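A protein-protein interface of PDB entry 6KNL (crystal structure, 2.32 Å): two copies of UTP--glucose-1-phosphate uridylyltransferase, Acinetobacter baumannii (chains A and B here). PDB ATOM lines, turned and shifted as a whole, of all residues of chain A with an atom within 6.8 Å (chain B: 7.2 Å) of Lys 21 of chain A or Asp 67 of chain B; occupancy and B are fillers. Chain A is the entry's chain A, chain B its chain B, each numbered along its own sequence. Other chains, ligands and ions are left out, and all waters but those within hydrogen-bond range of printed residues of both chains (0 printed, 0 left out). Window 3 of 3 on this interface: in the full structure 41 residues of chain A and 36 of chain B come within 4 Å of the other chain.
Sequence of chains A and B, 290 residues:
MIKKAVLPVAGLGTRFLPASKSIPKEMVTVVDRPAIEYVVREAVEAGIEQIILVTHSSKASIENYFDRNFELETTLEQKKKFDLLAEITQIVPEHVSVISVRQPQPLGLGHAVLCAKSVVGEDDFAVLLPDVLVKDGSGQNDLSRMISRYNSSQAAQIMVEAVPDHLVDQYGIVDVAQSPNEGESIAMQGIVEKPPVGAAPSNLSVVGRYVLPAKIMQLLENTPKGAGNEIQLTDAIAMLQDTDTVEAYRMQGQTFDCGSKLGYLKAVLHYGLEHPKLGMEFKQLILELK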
ATOM      1  N   LEU A  12     -28.621  10.726 -23.237  1.00  0.00           N
ATOM      2  CA  LEU A  12     -28.841  10.628 -21.769  1.00  0.00           C
ATOM      3  C   LEU A  12     -27.949   9.543 -21.165  1.00  0.00           C
ATOM      4  O   LEU A  12     -27.828   9.515 -19.917  1.00  0.00           O
ATOM      5  CB  LEU A  12     -30.319  10.322 -21.506  1.00  0.00           C
ATOM      6  CG  LEU A  12     -31.176  11.511 -21.090  1.00  0.00           C
ATOM      7  CD1 LEU A  12     -30.725  12.789 -21.777  1.00  0.00           C
ATOM      8  CD2 LEU A  12     -32.643  11.243 -21.373  1.00  0.00           C
ATOM      9  N   GLY A  13     -27.385   8.666 -22.002  1.00  0.00           N
ATOM     10  CA  GLY A  13     -26.464   7.602 -21.552  1.00  0.00           C
ATOM     11  C   GLY A  13     -27.123   6.664 -20.555  1.00  0.00           C
ATOM     12  O   GLY A  13     -26.763   6.709 -19.346  1.00  0.00           O
ATOM     13  N   PHE A  16     -24.643   3.740 -18.721  1.00  0.00           N
ATOM     14  CA  PHE A  16     -23.825   3.929 -17.490  1.00  0.00           C
ATOM     15  C   PHE A  16     -24.662   4.586 -16.392  1.00  0.00           C
ATOM     16  O   PHE A  16     -24.310   5.664 -15.868  1.00  0.00           O
ATOM     17  CB  PHE A  16     -22.515   4.677 -17.760  1.00  0.00           C
ATOM     18  CG  PHE A  16     -21.441   4.452 -16.718  1.00  0.00           C
ATOM     19  CD1 PHE A  16     -21.589   3.504 -15.712  1.00  0.00           C
ATOM     20  CD2 PHE A  16     -20.257   5.170 -16.759  1.00  0.00           C
ATOM     21  CE1 PHE A  16     -20.593   3.294 -14.769  1.00  0.00           C
ATOM     22  CE2 PHE A  16     -19.261   4.958 -15.814  1.00  0.00           C
ATOM     23  CZ  PHE A  16     -19.430   4.023 -14.820  1.00  0.00           C
ATOM     24  N   LEU A  17     -25.741   3.899 -16.039  1.00  0.00           N
ATOM     25  CA  LEU A  17     -26.599   4.196 -14.868  1.00  0.00           C
ATOM     26  C   LEU A  17     -26.133   3.268 -13.756  1.00  0.00           C
ATOM     27  O   LEU A  17     -25.612   2.201 -14.042  1.00  0.00           O
ATOM     28  CB  LEU A  17     -28.055   3.922 -15.249  1.00  0.00           C
ATOM     29  CG  LEU A  17     -28.981   5.113 -15.474  1.00  0.00           C
ATOM     30  CD1 LEU A  17     -28.259   6.351 -15.937  1.00  0.00           C
ATOM     31  CD2 LEU A  17     -30.076   4.750 -16.464  1.00  0.00           C
ATOM     32  N   PRO A  18     -26.287   3.612 -12.463  1.00  0.00           N
ATOM     33  CA  PRO A  18     -26.880   4.885 -12.046  1.00  0.00           C
ATOM     34  C   PRO A  18     -25.897   6.070 -12.013  1.00  0.00           C
ATOM     35  O   PRO A  18     -26.334   7.204 -11.737  1.00  0.00           O
ATOM     36  CB  PRO A  18     -27.360   4.537 -10.627  1.00  0.00           C
ATOM     37  CG  PRO A  18     -26.310   3.552 -10.120  1.00  0.00           C
ATOM     38  CD  PRO A  18     -25.925   2.740 -11.333  1.00  0.00           C
ATOM     39  N   ALA A  19     -24.615   5.804 -12.297  1.00  0.00           N
ATOM     40  CA  ALA A  19     -23.520   6.805 -12.277  1.00  0.00           C
ATOM     41  C   ALA A  19     -23.974   8.098 -12.958  1.00  0.00           C
ATOM     42  O   ALA A  19     -23.644   9.166 -12.435  1.00  0.00           O
ATOM     43  CB  ALA A  19     -22.273   6.261 -12.937  1.00  0.00           C
ATOM     44  N   SER A  20     -24.709   7.998 -14.071  1.00  0.00           N
ATOM     45  CA  SER A  20     -25.144   9.161 -14.889  1.00  0.00           C
ATOM     46  C   SER A  20     -26.620   9.462 -14.654  1.00  0.00           C
ATOM     47  O   SER A  20     -27.238  10.103 -15.512  1.00  0.00           O
ATOM     48  CB  SER A  20     -24.869   8.934 -16.352  1.00  0.00           C
ATOM     49  OG  SER A  20     -25.766   7.971 -16.878  1.00  0.00           O
ATOM     50  N   LYS A  21     -27.187   9.046 -13.524  1.00  0.00           N
ATOM     51  CA  LYS A  21     -28.598   9.401 -13.260  1.00  0.00           C
ATOM     52  C   LYS A  21     -28.686  10.921 -13.270  1.00  0.00           C
ATOM     53  O   LYS A  21     -29.456  11.438 -14.086  1.00  0.00           O
ATOM     54  CB  LYS A  21     -29.136   8.821 -11.954  1.00  0.00           C
ATOM     55  CG  LYS A  21     -30.578   9.218 -11.689  1.00  0.00           C
ATOM     56  CD  LYS A  21     -31.144   8.755 -10.381  1.00  0.00           C
ATOM     57  CE  LYS A  21     -32.447   9.468 -10.091  1.00  0.00           C
ATOM     58  NZ  LYS A  21     -33.076   8.954  -8.856  1.00  0.00           N
ATOM     59  N   SER A  22     -27.861  11.594 -12.456  1.00  0.00           N
ATOM     60  CA  SER A  22     -28.039  13.026 -12.082  1.00  0.00           C
ATOM     61  C   SER A  22     -26.864  13.925 -12.476  1.00  0.00           C
ATOM     62  O   SER A  22     -26.951  15.105 -12.150  1.00  0.00           O
ATOM     63  CB  SER A  22     -28.314  13.143 -10.622  1.00  0.00           C
ATOM     64  OG  SER A  22     -29.567  12.542 -10.331  1.00  0.00           O
ATOM     65  N   ILE A  23     -25.834  13.401 -13.146  1.00  0.00           N
ATOM     66  CA  ILE A  23     -24.761  14.210 -13.814  1.00  0.00           C
ATOM     67  C   ILE A  23     -24.588  13.620 -15.205  1.00  0.00           C
ATOM     68  O   ILE A  23     -24.835  12.442 -15.374  1.00  0.00           O
ATOM     69  CB  ILE A  23     -23.401  14.171 -13.066  1.00  0.00           C
ATOM     70  CG1 ILE A  23     -22.675  12.852 -13.360  1.00  0.00           C
ATOM     71  CG2 ILE A  23     -23.559  14.444 -11.573  1.00  0.00           C
ATOM     72  CD1 ILE A  23     -21.524  12.529 -12.458  1.00  0.00           C
ATOM     73  N   PRO A  24     -24.077  14.361 -16.210  1.00  0.00           N
ATOM     74  CA  PRO A  24     -23.872  13.785 -17.535  1.00  0.00           C
ATOM     75  C   PRO A  24     -22.842  12.648 -17.537  1.00  0.00           C
ATOM     76  O   PRO A  24     -21.871  12.742 -16.828  1.00  0.00           O
ATOM     77  CB  PRO A  24     -23.330  14.976 -18.337  1.00  0.00           C
ATOM     78  CG  PRO A  24     -23.829  16.185 -17.594  1.00  0.00           C
ATOM     79  CD  PRO A  24     -23.675  15.773 -16.147  1.00  0.00           C
ATOM     80  N   MET B  27     -20.819  13.667  -5.836  1.00  0.00           N
ATOM     81  CA  MET B  27     -21.370  12.970  -7.035  1.00  0.00           C
ATOM     82  C   MET B  27     -20.266  12.278  -7.848  1.00  0.00           C
ATOM     83  O   MET B  27     -20.568  11.660  -8.906  1.00  0.00           O
ATOM     84  CB  MET B  27     -22.113  13.973  -7.920  1.00  0.00           C
ATOM     85  CG  MET B  27     -23.373  14.468  -7.255  1.00  0.00           C
ATOM     86  SD  MET B  27     -24.334  13.055  -6.645  1.00  0.00           S
ATOM     87  CE  MET B  27     -24.947  12.470  -8.222  1.00  0.00           C
ATOM     88  N   PRO B  34     -22.418   7.484  -7.681  1.00  0.00           N
ATOM     89  CA  PRO B  34     -21.778   8.586  -6.982  1.00  0.00           C
ATOM     90  C   PRO B  34     -21.379   8.084  -5.589  1.00  0.00           C
ATOM     91  O   PRO B  34     -22.018   7.167  -5.075  1.00  0.00           O
ATOM     92  CB  PRO B  34     -22.829   9.705  -6.979  1.00  0.00           C
ATOM     93  CG  PRO B  34     -24.148   8.980  -7.116  1.00  0.00           C
ATOM     94  CD  PRO B  34     -23.837   7.745  -7.946  1.00  0.00           C
ATOM     95  N   SER B  61     -27.636  18.389  -7.953  1.00  0.00           N
ATOM     96  CA  SER B  61     -27.437  17.060  -8.565  1.00  0.00           C
ATOM     97  C   SER B  61     -27.504  15.993  -7.461  1.00  0.00           C
ATOM     98  O   SER B  61     -27.994  14.894  -7.756  1.00  0.00           O
ATOM     99  CB  SER B  61     -26.187  17.002  -9.424  1.00  0.00           C
ATOM    100  OG  SER B  61     -25.015  16.755  -8.676  1.00  0.00           O
ATOM    101  N   ILE B  62     -27.108  16.312  -6.220  1.00  0.00           N
ATOM    102  CA  ILE B  62     -27.236  15.356  -5.079  1.00  0.00           C
ATOM    103  C   ILE B  62     -28.727  15.146  -4.784  1.00  0.00           C
ATOM    104  O   ILE B  62     -29.141  13.981  -4.652  1.00  0.00           O
ATOM    105  CB  ILE B  62     -26.519  15.829  -3.797  1.00  0.00           C
ATOM    106  CG1 ILE B  62     -25.037  16.134  -4.008  1.00  0.00           C
ATOM    107  CG2 ILE B  62     -26.725  14.808  -2.686  1.00  0.00           C
ATOM    108  CD1 ILE B  62     -24.359  16.695  -2.764  1.00  0.00           C
ATOM    109  N   GLU B  63     -29.489  16.225  -4.599  1.00  0.00           N
ATOM    110  CA  GLU B  63     -30.927  16.105  -4.264  1.00  0.00           C
ATOM    111  C   GLU B  63     -31.589  15.288  -5.388  1.00  0.00           C
ATOM    112  O   GLU B  63     -32.214  14.261  -5.088  1.00  0.00           O
ATOM    113  CB  GLU B  63     -31.512  17.490  -4.011  1.00  0.00           C
ATOM    114  CG  GLU B  63     -31.035  18.085  -2.688  1.00  0.00           C
ATOM    115  CD  GLU B  63     -30.444  19.489  -2.764  1.00  0.00           C
ATOM    116  OE1 GLU B  63     -29.180  19.648  -2.576  1.00  0.00           O
ATOM    117  OE2 GLU B  63     -31.233  20.426  -3.011  1.00  0.00           O
ATOM    118  N   ASN B  64     -31.342  15.668  -6.643  1.00  0.00           N
ATOM    119  CA  ASN B  64     -31.910  15.030  -7.861  1.00  0.00           C
ATOM    120  C   ASN B  64     -31.655  13.519  -7.853  1.00  0.00           C
ATOM    121  O   ASN B  64     -32.514  12.787  -8.372  1.00  0.00           O
ATOM    122  CB  ASN B  64     -31.326  15.664  -9.122  1.00  0.00           C
ATOM    123  CG  ASN B  64     -31.792  17.092  -9.279  1.00  0.00           C
ATOM    124  OD1 ASN B  64     -32.797  17.485  -8.687  1.00  0.00           O
ATOM    125  ND2 ASN B  64     -31.076  17.872 -10.068  1.00  0.00           N
ATOM    126  N   TYR B  65     -30.512  13.080  -7.319  1.00  0.00           N
ATOM    127  CA  TYR B  65     -30.062  11.669  -7.380  1.00  0.00           C
ATOM    128  C   TYR B  65     -31.025  10.796  -6.564  1.00  0.00           C
ATOM    129  O   TYR B  65     -31.247   9.613  -6.940  1.00  0.00           O
ATOM    130  CB  TYR B  65     -28.609  11.524  -6.916  1.00  0.00           C
ATOM    131  CG  TYR B  65     -28.063  10.131  -7.090  1.00  0.00           C
ATOM    132  CD1 TYR B  65     -27.622   9.690  -8.325  1.00  0.00           C
ATOM    133  CD2 TYR B  65     -28.063   9.223  -6.044  1.00  0.00           C
ATOM    134  CE1 TYR B  65     -27.160   8.397  -8.518  1.00  0.00           C
ATOM    135  CE2 TYR B  65     -27.596   7.933  -6.214  1.00  0.00           C
ATOM    136  CZ  TYR B  65     -27.131   7.517  -7.452  1.00  0.00           C
ATOM    137  OH  TYR B  65     -26.666   6.237  -7.633  1.00  0.00           O
ATOM    138  N   PHE B  66     -31.562  11.331  -5.465  1.00  0.00           N
ATOM    139  CA  PHE B  66     -32.514  10.590  -4.598  1.00  0.00           C
ATOM    140  C   PHE B  66     -33.939  11.026  -4.927  1.00  0.00           C
ATOM    141  O   PHE B  66     -34.851  10.692  -4.156  1.00  0.00           O
ATOM    142  CB  PHE B  66     -32.180  10.783  -3.119  1.00  0.00           C
ATOM    143  CG  PHE B  66     -30.782  10.346  -2.769  1.00  0.00           C
ATOM    144  CD1 PHE B  66     -30.487   9.008  -2.597  1.00  0.00           C
ATOM    145  CD2 PHE B  66     -29.755  11.274  -2.658  1.00  0.00           C
ATOM    146  CE1 PHE B  66     -29.197   8.600  -2.297  1.00  0.00           C
ATOM    147  CE2 PHE B  66     -28.468  10.863  -2.353  1.00  0.00           C
ATOM    148  CZ  PHE B  66     -28.194   9.527  -2.163  1.00  0.00           C
ATOM    149  N   ASP B  67     -34.119  11.742  -6.036  1.00  0.00           N
ATOM    150  CA  ASP B  67     -35.458  12.145  -6.526  1.00  0.00           C
ATOM    151  C   ASP B  67     -35.724  11.301  -7.766  1.00  0.00           C
ATOM    152  O   ASP B  67     -34.846  10.482  -8.102  1.00  0.00           O
ATOM    153  CB  ASP B  67     -35.550  13.650  -6.776  1.00  0.00           C
ATOM    154  CG  ASP B  67     -36.980  14.143  -6.899  1.00  0.00           C
ATOM    155  OD1 ASP B  67     -37.888  13.294  -6.821  1.00  0.00           O
ATOM    156  OD2 ASP B  67     -37.180  15.350  -7.096  1.00  0.00           O
ATOM    157  N   ARG B  68     -36.874  11.498  -8.411  1.00  0.00           N
ATOM    158  CA  ARG B  68     -37.192  10.848  -9.706  1.00  0.00           C
ATOM    159  C   ARG B  68     -36.934  11.833 -10.844  1.00  0.00           C
ATOM    160  O   ARG B  68     -37.057  13.070 -10.634  1.00  0.00           O
ATOM    161  CB  ARG B  68     -38.603  10.272  -9.649  1.00  0.00           C
ATOM    162  CG  ARG B  68     -38.662   9.196  -8.578  1.00  0.00           C
ATOM    163  CD  ARG B  68     -39.915   8.379  -8.511  1.00  0.00           C
ATOM    164  NE  ARG B  68     -40.106   7.612  -9.719  1.00  0.00           N
ATOM    165  CZ  ARG B  68     -41.122   6.793  -9.899  1.00  0.00           C
ATOM    166  NH1 ARG B  68     -42.013   6.639  -8.931  1.00  0.00           N
ATOM    167  NH2 ARG B  68     -41.244   6.143 -11.043  1.00  0.00           N
ATOM    168  N   ASN B  69     -36.525  11.263 -11.979  1.00  0.00           N
ATOM    169  CA  ASN B  69     -36.102  11.986 -13.201  1.00  0.00           C
ATOM    170  C   ASN B  69     -37.061  11.531 -14.305  1.00  0.00           C
ATOM    171  O   ASN B  69     -36.854  10.419 -14.855  1.00  0.00           O
ATOM    172  CB  ASN B  69     -34.605  11.746 -13.425  1.00  0.00           C
ATOM    173  CG  ASN B  69     -34.061  12.216 -14.759  1.00  0.00           C
ATOM    174  OD1 ASN B  69     -34.816  12.543 -15.685  1.00  0.00           O
ATOM    175  ND2 ASN B  69     -32.736  12.227 -14.865  1.00  0.00           N
ATOM    176  N   LEU B  72     -35.757  10.712 -18.019  1.00  0.00           N
ATOM    177  CA  LEU B  72     -34.829   9.544 -18.035  1.00  0.00           C
ATOM    178  C   LEU B  72     -35.647   8.268 -17.877  1.00  0.00           C
ATOM    179  O   LEU B  72     -35.337   7.294 -18.561  1.00  0.00           O
ATOM    180  CB  LEU B  72     -33.786   9.658 -16.915  1.00  0.00           C
ATOM    181  CG  LEU B  72     -32.810   8.488 -16.801  1.00  0.00           C
ATOM    182  CD1 LEU B  72     -32.004   8.306 -18.072  1.00  0.00           C
ATOM    183  CD2 LEU B  72     -31.867   8.667 -15.618  1.00  0.00           C
ATOM    184  N   GLU B  73     -36.617   8.272 -16.965  1.00  0.00           N
ATOM    185  CA  GLU B  73     -37.437   7.077 -16.640  1.00  0.00           C
ATOM    186  C   GLU B  73     -38.272   6.655 -17.854  1.00  0.00           C
ATOM    187  O   GLU B  73     -38.349   5.446 -18.088  1.00  0.00           O
ATOM    188  CB  GLU B  73     -38.329   7.349 -15.432  1.00  0.00           C
ATOM    189  CG  GLU B  73     -37.603   7.127 -14.125  1.00  0.00           C
ATOM    190  CD  GLU B  73     -38.342   7.669 -12.922  1.00  0.00           C
ATOM    191  OE1 GLU B  73     -39.586   7.660 -12.947  1.00  0.00           O
ATOM    192  OE2 GLU B  73     -37.663   8.113 -11.971  1.00  0.00           O
ATOM    193  N   GLU B  87     -33.156   0.177 -10.663  1.00  0.00           N
ATOM    194  CA  GLU B  87     -31.889   0.615 -10.023  1.00  0.00           C
ATOM    195  C   GLU B  87     -31.869   2.146  -9.841  1.00  0.00           C
ATOM    196  O   GLU B  87     -31.097   2.596  -8.975  1.00  0.00           O
ATOM    197  CB  GLU B  87     -30.698   0.105 -10.849  1.00  0.00           C
ATOM    198  CG  GLU B  87     -29.333   0.661 -10.440  1.00  0.00           C
ATOM    199  CD  GLU B  87     -28.424  -0.263  -9.639  1.00  0.00           C
ATOM    200  OE1 GLU B  87     -27.819  -1.167 -10.265  1.00  0.00           O
ATOM    201  OE2 GLU B  87     -28.301  -0.066  -8.401  1.00  0.00           O
ATOM    202  N   ILE B  88     -32.660   2.938 -10.583  1.00  0.00           N
ATOM    203  CA  ILE B  88     -32.668   4.428 -10.414  1.00  0.00           C
ATOM    204  C   ILE B  88     -33.921   4.938  -9.688  1.00  0.00           C
ATOM    205  O   ILE B  88     -33.944   6.148  -9.414  1.00  0.00           O
ATOM    206  CB  ILE B  88     -32.475   5.196 -11.733  1.00  0.00           C
ATOM    207  CG1 ILE B  88     -33.597   4.939 -12.737  1.00  0.00           C
ATOM    208  CG2 ILE B  88     -31.110   4.911 -12.322  1.00  0.00           C
ATOM    209  CD1 ILE B  88     -33.778   6.060 -13.735  1.00  0.00           C
ATOM    210  N   THR B  89     -34.929   4.105  -9.405  1.00  0.00           N
ATOM    211  CA  THR B  89     -36.181   4.569  -8.729  1.00  0.00           C
ATOM    212  C   THR B  89     -36.203   4.164  -7.248  1.00  0.00           C
ATOM    213  O   THR B  89     -36.760   4.931  -6.446  1.00  0.00           O
ATOM    214  CB  THR B  89     -37.461   4.095  -9.431  1.00  0.00           C
ATOM    215  OG1 THR B  89     -37.470   2.674  -9.539  1.00  0.00           O
ATOM    216  CG2 THR B  89     -37.630   4.703 -10.803  1.00  0.00           C
ATOM    217  N   GLN B  90     -35.655   3.008  -6.883  1.00  0.00           N
ATOM    218  CA  GLN B  90     -35.786   2.492  -5.493  1.00  0.00           C
ATOM    219  C   GLN B  90     -34.484   2.797  -4.737  1.00  0.00           C
ATOM    220  O   GLN B  90     -34.107   1.982  -3.880  1.00  0.00           O
ATOM    221  CB  GLN B  90     -36.166   1.002  -5.518  1.00  0.00           C
ATOM    222  N   ILE B  91     -33.837   3.938  -5.015  1.00  0.00           N
ATOM    223  CA  ILE B  91     -32.422   4.198  -4.598  1.00  0.00           C
ATOM    224  C   ILE B  91     -32.341   4.079  -3.072  1.00  0.00           C
ATOM    225  O   ILE B  91     -31.374   3.489  -2.585  1.00  0.00           O
ATOM    226  CB  ILE B  91     -31.889   5.565  -5.077  1.00  0.00           C
ATOM    227  CG1 ILE B  91     -32.031   5.771  -6.592  1.00  0.00           C
ATOM    228  CG2 ILE B  91     -30.450   5.749  -4.600  1.00  0.00           C
ATOM    229  CD1 ILE B  91     -30.727   5.796  -7.368  1.00  0.00           C
ATOM    230  N   VAL B  98     -35.293  12.330   2.218  1.00  0.00           N
ATOM    231  CA  VAL B  98     -34.086  13.188   2.021  1.00  0.00           C
ATOM    232  C   VAL B  98     -34.536  14.646   2.084  1.00  0.00           C
ATOM    233  O   VAL B  98     -35.329  15.008   1.216  1.00  0.00           O
ATOM    234  CB  VAL B  98     -33.393  12.874   0.688  1.00  0.00           C
ATOM    235  CG1 VAL B  98     -32.101  13.649   0.550  1.00  0.00           C
ATOM    236  CG2 VAL B  98     -33.132  11.387   0.535  1.00  0.00           C
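NZ of Lys 21 of chain A sits at hydrogen-bond distance from O of Asp 67 of chain B. The backbone NH (N) of Tyr 65 of chain B sits close to the side-chain hydroxyl (OG) of Ser 22 of chain A (3.2 Å). The side-chain amino group of Lys 21 of chain A lies within hydrogen-bond range of the backbone carbonyl oxygen of Ile 88 of chain B (3.0 Å). The side-chain amide nitrogen (ND2) of Asn 69 of chain B sits at hydrogen-bond distance from the backbone carbonyl oxygen (O) of Lys 21 of chain A. The backbone carbonyl oxygen (O) of Tyr 65 of chain B lies within hydrogen-bond range of the side-chain amino group (NZ) of Lys 21 of chain A.
CG of Leu 17 of chain A touches CG2 of Ile 88 of chain B, 3.8 Å away. Tyr 65 of chain B touches Pro 18 of chain A. Lys 21 of chain A touches Asn 64 of chain B. CD2 of Leu 72 of chain B touches O of Lys 21 of chain A, 3.98 Å away. CB of Ser 22 of chain A touches O of Ser 61 of chain B (3.4 Å). Ser 22 of chain A touches Asn 64 of chain B. Met 27 of chain B touches Ile 23 of chain A. Ser 61 of chain B touches Ile 23 of chain A.
OD1 of Asn 69 of chain B lies within hydrogen-bond range of N of Leu 72 of chain B, at 3.1 Å. The side-chain carboxylate (OE2) of Glu 73 of chain B sits at hydrogen-bond distance from the backbone NH (N) of Asn 69 of chain B (3.3 Å).
No position is printed for both chains. Of the 13 pairs that touch across the chains among the printed residues, none has its exchanged pair printed and touching as well.
Lys 21 of chain A touches just these residues of chain B: Asn 64 (3.7 Å), Tyr 65 (2.7 Å), Asp 67 (2.5 Å), Asn 69 (3.5 Å), Leu 72 (3.98 Å) and Ile 88 (3.0 Å). Of chain A, only Lys 21 (2.5 Å) comes within 4 Å of Asp 67 of chain B. Printed residues of chain A within 4 Å of Leu 72 of chain B: Lys 21 (3.98 Å). Printed residues of chain A within 4 Å of Asn 64 of chain B: Lys 21 (3.7 Å) and Ser 22 (3.4 Å). Of the printed residues of chain A, Tyr 65 of chain B touches Pro 18, Lys 21 and Ser 22. Of the printed residues of chain A, Ser 61 of chain B touches Ser 22 and Ile 23. Leu 12 of chain A touches none of the printed residues of chain B. Ile 91 of chain B touches none of the printed residues of chain A. The nearest residue of chain B that does not touch Lys 21 of chain A is Ile 91 of chain B (4.04 Å). The nearest residue of chain A that does not touch Asp 67 of chain B is Ser 22 of chain A (6.1 Å). The nearest printed residue of chain B that does not touch Ile 23 of chain A is Pro 34 of chain B (6.3 Å).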
